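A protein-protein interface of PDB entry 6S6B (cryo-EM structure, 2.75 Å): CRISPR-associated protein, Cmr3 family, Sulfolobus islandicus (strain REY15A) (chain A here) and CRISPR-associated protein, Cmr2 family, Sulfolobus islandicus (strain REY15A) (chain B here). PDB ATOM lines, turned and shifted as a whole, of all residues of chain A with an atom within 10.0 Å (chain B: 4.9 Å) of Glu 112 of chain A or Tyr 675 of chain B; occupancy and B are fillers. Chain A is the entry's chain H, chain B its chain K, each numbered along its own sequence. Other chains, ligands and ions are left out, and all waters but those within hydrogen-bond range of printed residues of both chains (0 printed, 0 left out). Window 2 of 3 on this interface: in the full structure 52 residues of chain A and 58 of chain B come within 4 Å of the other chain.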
ATOM      1  N   LEU A 106     -34.227  25.721 -17.401  1.00  0.00           N
ATOM      2  CA  LEU A 106     -32.819  25.452 -17.145  1.00  0.00           C
ATOM      3  C   LEU A 106     -32.311  24.320 -18.024  1.00  0.00           C
ATOM      4  O   LEU A 106     -31.263  24.440 -18.667  1.00  0.00           O
ATOM      5  CB  LEU A 106     -32.610  25.120 -15.671  1.00  0.00           C
ATOM      6  CG  LEU A 106     -31.224  24.632 -15.279  1.00  0.00           C
ATOM      7  CD1 LEU A 106     -30.204  25.716 -15.545  1.00  0.00           C
ATOM      8  CD2 LEU A 106     -31.216  24.232 -13.821  1.00  0.00           C
ATOM      9  N   GLU A 108     -33.043  23.481 -20.788  1.00  0.00           N
ATOM     10  CA  GLU A 108     -33.062  23.814 -22.201  1.00  0.00           C
ATOM     11  C   GLU A 108     -32.065  24.906 -22.554  1.00  0.00           C
ATOM     12  O   GLU A 108     -31.907  25.224 -23.737  1.00  0.00           O
ATOM     13  CB  GLU A 108     -34.483  24.226 -22.617  1.00  0.00           C
ATOM     14  CG  GLU A 108     -34.706  24.406 -24.114  1.00  0.00           C
ATOM     15  CD  GLU A 108     -34.511  23.119 -24.900  1.00  0.00           C
ATOM     16  OE1 GLU A 108     -34.682  22.029 -24.315  1.00  0.00           O
ATOM     17  OE2 GLU A 108     -34.185  23.199 -26.103  1.00  0.00           O
ATOM     18  N   LYS A 109     -31.360  25.465 -21.574  1.00  0.00           N
ATOM     19  CA  LYS A 109     -30.429  26.546 -21.847  1.00  0.00           C
ATOM     20  C   LYS A 109     -29.280  26.061 -22.721  1.00  0.00           C
ATOM     21  O   LYS A 109     -29.166  24.883 -23.059  1.00  0.00           O
ATOM     22  CB  LYS A 109     -29.870  27.119 -20.550  1.00  0.00           C
ATOM     23  CG  LYS A 109     -30.873  27.866 -19.720  1.00  0.00           C
ATOM     24  CD  LYS A 109     -30.202  28.502 -18.531  1.00  0.00           C
ATOM     25  CE  LYS A 109     -31.217  29.180 -17.644  1.00  0.00           C
ATOM     26  NZ  LYS A 109     -31.858  30.324 -18.339  1.00  0.00           N
ATOM     27  N   GLU A 110     -28.417  27.000 -23.091  1.00  0.00           N
ATOM     28  CA  GLU A 110     -27.240  26.644 -23.857  1.00  0.00           C
ATOM     29  C   GLU A 110     -26.342  25.735 -23.024  1.00  0.00           C
ATOM     30  O   GLU A 110     -26.536  25.557 -21.821  1.00  0.00           O
ATOM     31  CB  GLU A 110     -26.479  27.892 -24.296  1.00  0.00           C
ATOM     32  CG  GLU A 110     -25.620  28.505 -23.208  1.00  0.00           C
ATOM     33  CD  GLU A 110     -24.518  29.387 -23.764  1.00  0.00           C
ATOM     34  OE1 GLU A 110     -24.722  29.994 -24.835  1.00  0.00           O
ATOM     35  OE2 GLU A 110     -23.444  29.467 -23.131  1.00  0.00           O
ATOM     36  N   TYR A 111     -25.342  25.158 -23.689  1.00  0.00           N
ATOM     37  CA  TYR A 111     -24.493  24.162 -23.049  1.00  0.00           C
ATOM     38  C   TYR A 111     -23.902  24.682 -21.746  1.00  0.00           C
ATOM     39  O   TYR A 111     -24.136  24.118 -20.673  1.00  0.00           O
ATOM     40  CB  TYR A 111     -23.389  23.729 -24.012  1.00  0.00           C
ATOM     41  CG  TYR A 111     -22.173  23.150 -23.331  1.00  0.00           C
ATOM     42  CD1 TYR A 111     -22.281  22.071 -22.469  1.00  0.00           C
ATOM     43  CD2 TYR A 111     -20.913  23.669 -23.570  1.00  0.00           C
ATOM     44  CE1 TYR A 111     -21.178  21.548 -21.848  1.00  0.00           C
ATOM     45  CE2 TYR A 111     -19.803  23.144 -22.958  1.00  0.00           C
ATOM     46  CZ  TYR A 111     -19.941  22.084 -22.098  1.00  0.00           C
ATOM     47  OH  TYR A 111     -18.833  21.555 -21.484  1.00  0.00           O
ATOM     48  N   GLU A 112     -23.141  25.772 -21.819  1.00  0.00           N
ATOM     49  CA  GLU A 112     -22.393  26.209 -20.649  1.00  0.00           C
ATOM     50  C   GLU A 112     -23.301  26.773 -19.567  1.00  0.00           C
ATOM     51  O   GLU A 112     -23.008  26.622 -18.377  1.00  0.00           O
ATOM     52  CB  GLU A 112     -21.352  27.241 -21.053  1.00  0.00           C
ATOM     53  CG  GLU A 112     -20.116  27.165 -20.208  1.00  0.00           C
ATOM     54  CD  GLU A 112     -19.417  25.835 -20.349  1.00  0.00           C
ATOM     55  OE1 GLU A 112     -18.825  25.592 -21.419  1.00  0.00           O
ATOM     56  OE2 GLU A 112     -19.462  25.031 -19.395  1.00  0.00           O
ATOM     57  N   ARG A 113     -24.391  27.430 -19.952  1.00  0.00           N
ATOM     58  CA  ARG A 113     -25.320  27.961 -18.966  1.00  0.00           C
ATOM     59  C   ARG A 113     -26.161  26.874 -18.323  1.00  0.00           C
ATOM     60  O   ARG A 113     -26.675  27.076 -17.220  1.00  0.00           O
ATOM     61  CB  ARG A 113     -26.231  29.005 -19.612  1.00  0.00           C
ATOM     62  CG  ARG A 113     -25.524  30.294 -19.976  1.00  0.00           C
ATOM     63  CD  ARG A 113     -25.800  31.372 -18.954  1.00  0.00           C
ATOM     64  NE  ARG A 113     -27.229  31.622 -18.804  1.00  0.00           N
ATOM     65  CZ  ARG A 113     -27.872  32.638 -19.368  1.00  0.00           C
ATOM     66  NH1 ARG A 113     -29.175  32.790 -19.180  1.00  0.00           N
ATOM     67  NH2 ARG A 113     -27.210  33.506 -20.121  1.00  0.00           N
ATOM     68  N   ARG A 114     -26.316  25.730 -18.988  1.00  0.00           N
ATOM     69  CA  ARG A 114     -27.054  24.623 -18.394  1.00  0.00           C
ATOM     70  C   ARG A 114     -26.237  23.950 -17.302  1.00  0.00           C
ATOM     71  O   ARG A 114     -26.736  23.712 -16.198  1.00  0.00           O
ATOM     72  CB  ARG A 114     -27.439  23.617 -19.473  1.00  0.00           C
ATOM     73  CG  ARG A 114     -28.219  22.433 -18.966  1.00  0.00           C
ATOM     74  CD  ARG A 114     -28.357  21.391 -20.053  1.00  0.00           C
ATOM     75  NE  ARG A 114     -27.062  20.855 -20.454  1.00  0.00           N
ATOM     76  CZ  ARG A 114     -26.607  20.856 -21.703  1.00  0.00           C
ATOM     77  NH1 ARG A 114     -25.416  20.347 -21.973  1.00  0.00           N
ATOM     78  NH2 ARG A 114     -27.339  21.368 -22.679  1.00  0.00           N
ATOM     79  N   GLU A 115     -24.976  23.637 -17.597  1.00  0.00           N
ATOM     80  CA  GLU A 115     -24.130  22.961 -16.622  1.00  0.00           C
ATOM     81  C   GLU A 115     -24.000  23.776 -15.345  1.00  0.00           C
ATOM     82  O   GLU A 115     -24.109  23.237 -14.239  1.00  0.00           O
ATOM     83  CB  GLU A 115     -22.756  22.685 -17.226  1.00  0.00           C
ATOM     84  CG  GLU A 115     -22.801  22.075 -18.611  1.00  0.00           C
ATOM     85  CD  GLU A 115     -23.668  20.833 -18.675  1.00  0.00           C
ATOM     86  OE1 GLU A 115     -23.610  20.010 -17.737  1.00  0.00           O
ATOM     87  OE2 GLU A 115     -24.408  20.678 -19.668  1.00  0.00           O
ATOM     88  N   LYS A 116     -23.765  25.081 -15.476  1.00  0.00           N
ATOM     89  CA  LYS A 116     -23.601  25.915 -14.292  1.00  0.00           C
ATOM     90  C   LYS A 116     -24.859  25.919 -13.440  1.00  0.00           C
ATOM     91  O   LYS A 116     -24.787  25.812 -12.212  1.00  0.00           O
ATOM     92  CB  LYS A 116     -23.231  27.339 -14.694  1.00  0.00           C
ATOM     93  CG  LYS A 116     -23.301  28.314 -13.541  1.00  0.00           C
ATOM     94  CD  LYS A 116     -22.945  29.716 -13.972  1.00  0.00           C
ATOM     95  CE  LYS A 116     -22.914  30.644 -12.779  1.00  0.00           C
ATOM     96  NZ  LYS A 116     -22.345  29.959 -11.586  1.00  0.00           N
ATOM     97  N   GLY A 117     -26.024  26.045 -14.073  1.00  0.00           N
ATOM     98  CA  GLY A 117     -27.260  26.047 -13.312  1.00  0.00           C
ATOM     99  C   GLY A 117     -27.508  24.722 -12.621  1.00  0.00           C
ATOM    100  O   GLY A 117     -27.899  24.680 -11.452  1.00  0.00           O
ATOM    101  N   ILE A 118     -27.280  23.622 -13.336  1.00  0.00           N
ATOM    102  CA  ILE A 118     -27.456  22.295 -12.752  1.00  0.00           C
ATOM    103  C   ILE A 118     -26.449  22.068 -11.633  1.00  0.00           C
ATOM    104  O   ILE A 118     -26.799  21.598 -10.545  1.00  0.00           O
ATOM    105  CB  ILE A 118     -27.341  21.219 -13.843  1.00  0.00           C
ATOM    106  CG1 ILE A 118     -28.700  20.988 -14.498  1.00  0.00           C
ATOM    107  CG2 ILE A 118     -26.787  19.930 -13.276  1.00  0.00           C
ATOM    108  CD1 ILE A 118     -28.613  20.283 -15.816  1.00  0.00           C
ATOM    109  N   TYR A 119     -25.183  22.402 -11.888  1.00  0.00           N
ATOM    110  CA  TYR A 119     -24.133  22.194 -10.897  1.00  0.00           C
ATOM    111  C   TYR A 119     -24.474  22.873  -9.579  1.00  0.00           C
ATOM    112  O   TYR A 119     -24.285  22.300  -8.502  1.00  0.00           O
ATOM    113  CB  TYR A 119     -22.802  22.710 -11.446  1.00  0.00           C
ATOM    114  CG  TYR A 119     -21.680  22.776 -10.438  1.00  0.00           C
ATOM    115  CD1 TYR A 119     -21.497  23.899  -9.642  1.00  0.00           C
ATOM    116  CD2 TYR A 119     -20.790  21.723 -10.296  1.00  0.00           C
ATOM    117  CE1 TYR A 119     -20.472  23.963  -8.725  1.00  0.00           C
ATOM    118  CE2 TYR A 119     -19.761  21.779  -9.384  1.00  0.00           C
ATOM    119  CZ  TYR A 119     -19.605  22.901  -8.602  1.00  0.00           C
ATOM    120  OH  TYR A 119     -18.580  22.961  -7.690  1.00  0.00           O
ATOM    121  N   GLU A 120     -24.986  24.099  -9.645  1.00  0.00           N
ATOM    122  CA  GLU A 120     -25.279  24.834  -8.425  1.00  0.00           C
ATOM    123  C   GLU A 120     -26.508  24.310  -7.702  1.00  0.00           C
ATOM    124  O   GLU A 120     -26.711  24.657  -6.536  1.00  0.00           O
ATOM    125  CB  GLU A 120     -25.452  26.315  -8.745  1.00  0.00           C
ATOM    126  CG  GLU A 120     -24.189  26.969  -9.280  1.00  0.00           C
ATOM    127  CD  GLU A 120     -23.066  27.008  -8.258  1.00  0.00           C
ATOM    128  OE1 GLU A 120     -23.358  27.124  -7.050  1.00  0.00           O
ATOM    129  OE2 GLU A 120     -21.889  26.923  -8.665  1.00  0.00           O
ATOM    130  N   GLU B 659     -11.673  20.844 -24.412  1.00  0.00           N
ATOM    131  CA  GLU B 659     -12.423  21.970 -24.943  1.00  0.00           C
ATOM    132  C   GLU B 659     -11.581  23.231 -25.052  1.00  0.00           C
ATOM    133  O   GLU B 659     -12.118  24.284 -25.404  1.00  0.00           O
ATOM    134  CB  GLU B 659     -13.639  22.251 -24.064  1.00  0.00           C
ATOM    135  CG  GLU B 659     -14.795  21.300 -24.257  1.00  0.00           C
ATOM    136  CD  GLU B 659     -15.896  21.527 -23.240  1.00  0.00           C
ATOM    137  OE1 GLU B 659     -15.718  21.126 -22.071  1.00  0.00           O
ATOM    138  OE2 GLU B 659     -16.936  22.113 -23.605  1.00  0.00           O
ATOM    139  N   LYS B 661     -10.419  24.920 -22.634  1.00  0.00           N
ATOM    140  CA  LYS B 661     -10.660  25.814 -21.517  1.00  0.00           C
ATOM    141  C   LYS B 661      -9.413  25.931 -20.646  1.00  0.00           C
ATOM    142  O   LYS B 661      -8.418  25.226 -20.832  1.00  0.00           O
ATOM    143  CB  LYS B 661     -11.841  25.325 -20.689  1.00  0.00           C
ATOM    144  CG  LYS B 661     -13.136  25.274 -21.459  1.00  0.00           C
ATOM    145  CD  LYS B 661     -14.257  24.782 -20.585  1.00  0.00           C
ATOM    146  CE  LYS B 661     -15.578  24.845 -21.307  1.00  0.00           C
ATOM    147  NZ  LYS B 661     -16.671  24.364 -20.430  1.00  0.00           N
ATOM    148  N   LEU B 662      -9.477  26.841 -19.679  1.00  0.00           N
ATOM    149  CA  LEU B 662      -8.342  27.144 -18.822  1.00  0.00           C
ATOM    150  C   LEU B 662      -8.547  26.684 -17.389  1.00  0.00           C
ATOM    151  O   LEU B 662      -7.721  26.998 -16.526  1.00  0.00           O
ATOM    152  CB  LEU B 662      -8.048  28.643 -18.847  1.00  0.00           C
ATOM    153  CG  LEU B 662      -7.695  29.234 -20.210  1.00  0.00           C
ATOM    154  CD1 LEU B 662      -7.087  30.600 -20.027  1.00  0.00           C
ATOM    155  CD2 LEU B 662      -6.750  28.333 -20.980  1.00  0.00           C
ATOM    156  N   THR B 663      -9.627  25.959 -17.108  1.00  0.00           N
ATOM    157  CA  THR B 663      -9.826  25.447 -15.756  1.00  0.00           C
ATOM    158  C   THR B 663      -8.703  24.535 -15.277  1.00  0.00           C
ATOM    159  O   THR B 663      -8.349  24.625 -14.090  1.00  0.00           O
ATOM    160  CB  THR B 663     -11.181  24.738 -15.650  1.00  0.00           C
ATOM    161  OG1 THR B 663     -11.284  23.732 -16.658  1.00  0.00           O
ATOM    162  CG2 THR B 663     -12.305  25.727 -15.822  1.00  0.00           C
ATOM    163  N   ILE B 670     -10.802  29.783 -11.302  1.00  0.00           N
ATOM    164  CA  ILE B 670     -11.923  29.761 -12.226  1.00  0.00           C
ATOM    165  C   ILE B 670     -12.412  28.325 -12.306  1.00  0.00           C
ATOM    166  O   ILE B 670     -11.610  27.387 -12.326  1.00  0.00           O
ATOM    167  CB  ILE B 670     -11.546  30.311 -13.617  1.00  0.00           C
ATOM    168  CG1 ILE B 670     -10.605  29.361 -14.355  1.00  0.00           C
ATOM    169  CG2 ILE B 670     -10.905  31.677 -13.490  1.00  0.00           C
ATOM    170  CD1 ILE B 670     -10.320  29.783 -15.767  1.00  0.00           C
ATOM    171  N   ASP B 671     -13.725  28.151 -12.296  1.00  0.00           N
ATOM    172  CA  ASP B 671     -14.324  26.831 -12.376  1.00  0.00           C
ATOM    173  C   ASP B 671     -15.053  26.678 -13.700  1.00  0.00           C
ATOM    174  O   ASP B 671     -15.315  27.655 -14.406  1.00  0.00           O
ATOM    175  CB  ASP B 671     -15.283  26.587 -11.209  1.00  0.00           C
ATOM    176  CG  ASP B 671     -16.281  27.711 -11.028  1.00  0.00           C
ATOM    177  OD1 ASP B 671     -16.284  28.644 -11.854  1.00  0.00           O
ATOM    178  OD2 ASP B 671     -17.060  27.663 -10.055  1.00  0.00           O
ATOM    179  N   SER B 672     -15.372  25.427 -14.031  1.00  0.00           N
ATOM    180  CA  SER B 672     -16.082  25.142 -15.273  1.00  0.00           C
ATOM    181  C   SER B 672     -17.324  26.007 -15.413  1.00  0.00           C
ATOM    182  O   SER B 672     -17.689  26.411 -16.522  1.00  0.00           O
ATOM    183  CB  SER B 672     -16.448  23.660 -15.325  1.00  0.00           C
ATOM    184  OG  SER B 672     -17.338  23.331 -14.278  1.00  0.00           O
ATOM    185  N   GLY B 673     -17.979  26.316 -14.293  1.00  0.00           N
ATOM    186  CA  GLY B 673     -19.152  27.167 -14.339  1.00  0.00           C
ATOM    187  C   GLY B 673     -18.857  28.580 -14.799  1.00  0.00           C
ATOM    188  O   GLY B 673     -19.739  29.261 -15.327  1.00  0.00           O
ATOM    189  N   ASP B 674     -17.619  29.043 -14.612  1.00  0.00           N
ATOM    190  CA  ASP B 674     -17.277  30.406 -15.002  1.00  0.00           C
ATOM    191  C   ASP B 674     -17.343  30.618 -16.505  1.00  0.00           C
ATOM    192  O   ASP B 674     -17.458  31.763 -16.947  1.00  0.00           O
ATOM    193  CB  ASP B 674     -15.884  30.778 -14.499  1.00  0.00           C
ATOM    194  CG  ASP B 674     -15.891  31.245 -13.062  1.00  0.00           C
ATOM    195  OD1 ASP B 674     -16.931  31.770 -12.610  1.00  0.00           O
ATOM    196  OD2 ASP B 674     -14.859  31.084 -12.381  1.00  0.00           O
ATOM    197  N   TYR B 675     -17.272  29.559 -17.299  1.00  0.00           N
ATOM    198  CA  TYR B 675     -17.280  29.732 -18.742  1.00  0.00           C
ATOM    199  C   TYR B 675     -18.662  30.035 -19.295  1.00  0.00           C
ATOM    200  O   TYR B 675     -18.792  30.266 -20.501  1.00  0.00           O
ATOM    201  CB  TYR B 675     -16.689  28.499 -19.421  1.00  0.00           C
ATOM    202  CG  TYR B 675     -15.202  28.622 -19.601  1.00  0.00           C
ATOM    203  CD1 TYR B 675     -14.328  28.243 -18.596  1.00  0.00           C
ATOM    204  CD2 TYR B 675     -14.671  29.152 -20.761  1.00  0.00           C
ATOM    205  CE1 TYR B 675     -12.973  28.370 -18.752  1.00  0.00           C
ATOM    206  CE2 TYR B 675     -13.318  29.281 -20.926  1.00  0.00           C
ATOM    207  CZ  TYR B 675     -12.472  28.891 -19.920  1.00  0.00           C
ATOM    208  OH  TYR B 675     -11.117  29.023 -20.091  1.00  0.00           O
ATOM    209  N   ALA B 676     -19.693  30.037 -18.450  1.00  0.00           N
ATOM    210  CA  ALA B 676     -20.975  30.594 -18.857  1.00  0.00           C
ATOM    211  C   ALA B 676     -20.902  32.106 -19.009  1.00  0.00           C
ATOM    212  O   ALA B 676     -21.731  32.690 -19.713  1.00  0.00           O
ATOM    213  CB  ALA B 676     -22.059  30.216 -17.849  1.00  0.00           C
ATOM    214  N   ASN B 677     -19.932  32.746 -18.356  1.00  0.00           N
ATOM    215  CA  ASN B 677     -19.679  34.170 -18.545  1.00  0.00           C
ATOM    216  C   ASN B 677     -18.201  34.393 -18.232  1.00  0.00           C
ATOM    217  O   ASN B 677     -17.830  34.530 -17.064  1.00  0.00           O
ATOM    218  CB  ASN B 677     -20.575  35.008 -17.652  1.00  0.00           C
ATOM    219  CG  ASN B 677     -20.416  36.492 -17.896  1.00  0.00           C
ATOM    220  OD1 ASN B 677     -19.852  36.912 -18.905  1.00  0.00           O
ATOM    221  ND2 ASN B 677     -20.914  37.296 -16.968  1.00  0.00           N
ATOM    222  N   ILE B 678     -17.373  34.437 -19.276  1.00  0.00           N
ATOM    223  CA  ILE B 678     -15.935  34.523 -19.052  1.00  0.00           C
ATOM    224  C   ILE B 678     -15.520  35.944 -18.693  1.00  0.00           C
ATOM    225  O   ILE B 678     -14.430  36.149 -18.148  1.00  0.00           O
ATOM    226  CB  ILE B 678     -15.155  34.034 -20.285  1.00  0.00           C
ATOM    227  CG1 ILE B 678     -15.658  32.666 -20.736  1.00  0.00           C
ATOM    228  CG2 ILE B 678     -13.688  33.872 -19.957  1.00  0.00           C
ATOM    229  CD1 ILE B 678     -16.717  32.722 -21.822  1.00  0.00           C
ATOM    230  N   VAL B 685      -8.162  35.158 -16.957  1.00  0.00           N
ATOM    231  CA  VAL B 685      -8.155  34.339 -18.165  1.00  0.00           C
ATOM    232  C   VAL B 685      -7.317  34.997 -19.247  1.00  0.00           C
ATOM    233  O   VAL B 685      -6.769  34.317 -20.121  1.00  0.00           O
ATOM    234  CB  VAL B 685      -9.596  34.077 -18.645  1.00  0.00           C
ATOM    235  CG1 VAL B 685     -10.283  35.370 -19.013  1.00  0.00           C
ATOM    236  CG2 VAL B 685      -9.605  33.120 -19.807  1.00  0.00           C
ATOM    237  N   GLU B 761     -13.344  34.286 -26.111  1.00  0.00           N
ATOM    238  CA  GLU B 761     -13.849  33.017 -25.607  1.00  0.00           C
ATOM    239  C   GLU B 761     -13.126  32.559 -24.352  1.00  0.00           C
ATOM    240  O   GLU B 761     -13.624  31.669 -23.656  1.00  0.00           O
ATOM    241  CB  GLU B 761     -13.735  31.940 -26.684  1.00  0.00           C
ATOM    242  CG  GLU B 761     -14.887  31.934 -27.663  1.00  0.00           C
ATOM    243  CD  GLU B 761     -16.214  31.644 -26.996  1.00  0.00           C
ATOM    244  OE1 GLU B 761     -16.393  30.519 -26.489  1.00  0.00           O
ATOM    245  OE2 GLU B 761     -17.080  32.541 -26.977  1.00  0.00           O
ATOM    246  N   GLY B 762     -11.973  33.144 -24.049  1.00  0.00           N
ATOM    247  CA  GLY B 762     -11.224  32.744 -22.876  1.00  0.00           C
ATOM    248  C   GLY B 762     -10.764  31.308 -22.902  1.00  0.00           C
ATOM    249  O   GLY B 762     -10.674  30.672 -21.848  1.00  0.00           O
ATOM    250  N   ARG B 763     -10.464  30.775 -24.082  1.00  0.00           N
ATOM    251  CA  ARG B 763     -10.066  29.383 -24.193  1.00  0.00           C
ATOM    252  C   ARG B 763      -9.335  29.177 -25.507  1.00  0.00           C
ATOM    253  O   ARG B 763      -9.624  29.840 -26.505  1.00  0.00           O
ATOM    254  CB  ARG B 763     -11.276  28.453 -24.104  1.00  0.00           C
ATOM    255  CG  ARG B 763     -12.376  28.799 -25.075  1.00  0.00           C
ATOM    256  CD  ARG B 763     -13.459  27.748 -25.071  1.00  0.00           C
ATOM    257  NE  ARG B 763     -14.335  27.882 -26.225  1.00  0.00           N
ATOM    258  CZ  ARG B 763     -14.015  27.485 -27.450  1.00  0.00           C
ATOM    259  NH1 ARG B 763     -14.873  27.643 -28.444  1.00  0.00           N
ATOM    260  NH2 ARG B 763     -12.841  26.921 -27.679  1.00  0.00           N
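The side-chain amino group (NZ) of Lys 661 of chain B lies within salt-bridge range of the side-chain carboxylate (OE1) of Glu 112 of chain A, 2.7 Å away. The side-chain hydroxyl (OH) of Tyr 111 of chain A is in hydrogen-bond range of the side-chain carboxylate (OE2) of Glu 659 of chain B, at 2.9 Å.
N of Leu 662 of chain B is in hydrogen-bond range of OH of Tyr 675 of chain B, 2.8 Å away. The backbone carbonyl oxygen (O) of Gly 762 of chain B lies within hydrogen-bond range of the side-chain hydroxyl (OH) of Tyr 675 of chain B (2.4 Å). OE1 of Glu 659 of chain B lies within salt-bridge range of NZ of Lys 661 of chain B (3.8 Å).
Lys 661 of chain B touches Tyr 111 of chain A. Glu 112 of chain A touches Ser 672 of chain B (OE2 to O, 3.6 Å). Glu 112 of chain A touches Tyr 675 of chain B (CG to C, 3.3 Å). CG of Glu 112 of chain A touches N of Ala 676 of chain B, at 3.4 Å. O of Gly 673 of chain B touches CD of Lys 116 of chain A, 3.5 Å away.
Of the printed residues of chain B, Tyr 111 of chain A touches Glu 659 and Lys 661. Glu 112 of chain A touches four residues of chain B. Arg 113 of chain A touches none of the printed residues of chain B. Of the printed residues of chain A, Lys 661 of chain B touches Tyr 111 (3.7 Å) and Glu 112 (2.7 Å). No residue of chain A comes within 4 Å of Leu 662 of chain B. Ser 672 of chain B touches just one residue of chain A: Glu 112 (3.6 Å). Gly 673 of chain B touches just one residue of chain A: Lys 116. No residue of chain A comes within 4 Å of Asp 674 of chain B. Of chain A, only Glu 112 (3.3 Å) comes within 4 Å of Tyr 675 of chain B. Printed residues of chain A within 4 Å of Ala 676 of chain B: Glu 112 (3.4 Å). The nearest residue of chain B that does not touch Glu 112 of chain A is Glu 659 of chain B (4.5 Å). The nearest residue of chain A that does not touch Tyr 675 of chain B is Glu 110 of chain A (5.4 Å).
Of the 14 printed residues of chain A, 3 touch a printed residue of chain B. Printed residues of chain A that touch a printed residue of chain B: Tyr 111, Glu 112 and Lys 116. Of the 17 printed residues of chain B, 6 touch a printed residue of chain A. Printed residues of chain B that touch a printed residue of chain A: Glu 659, Lys 661, Ser 672, Gly 673, Tyr 675 and Ala 676. Hydrophobic or aromatic side chains of chain B that line the printed part of chain A: Tyr 675 and Ala 676. Among the printed residues, 7 pairs touch across the chains. Among the printed residues, Asp or Glu carboxylates within 4 Å of a Lys or Arg side-chain nitrogen of the other chain: Glu 112 of chain A with Lys 661 of chain B.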
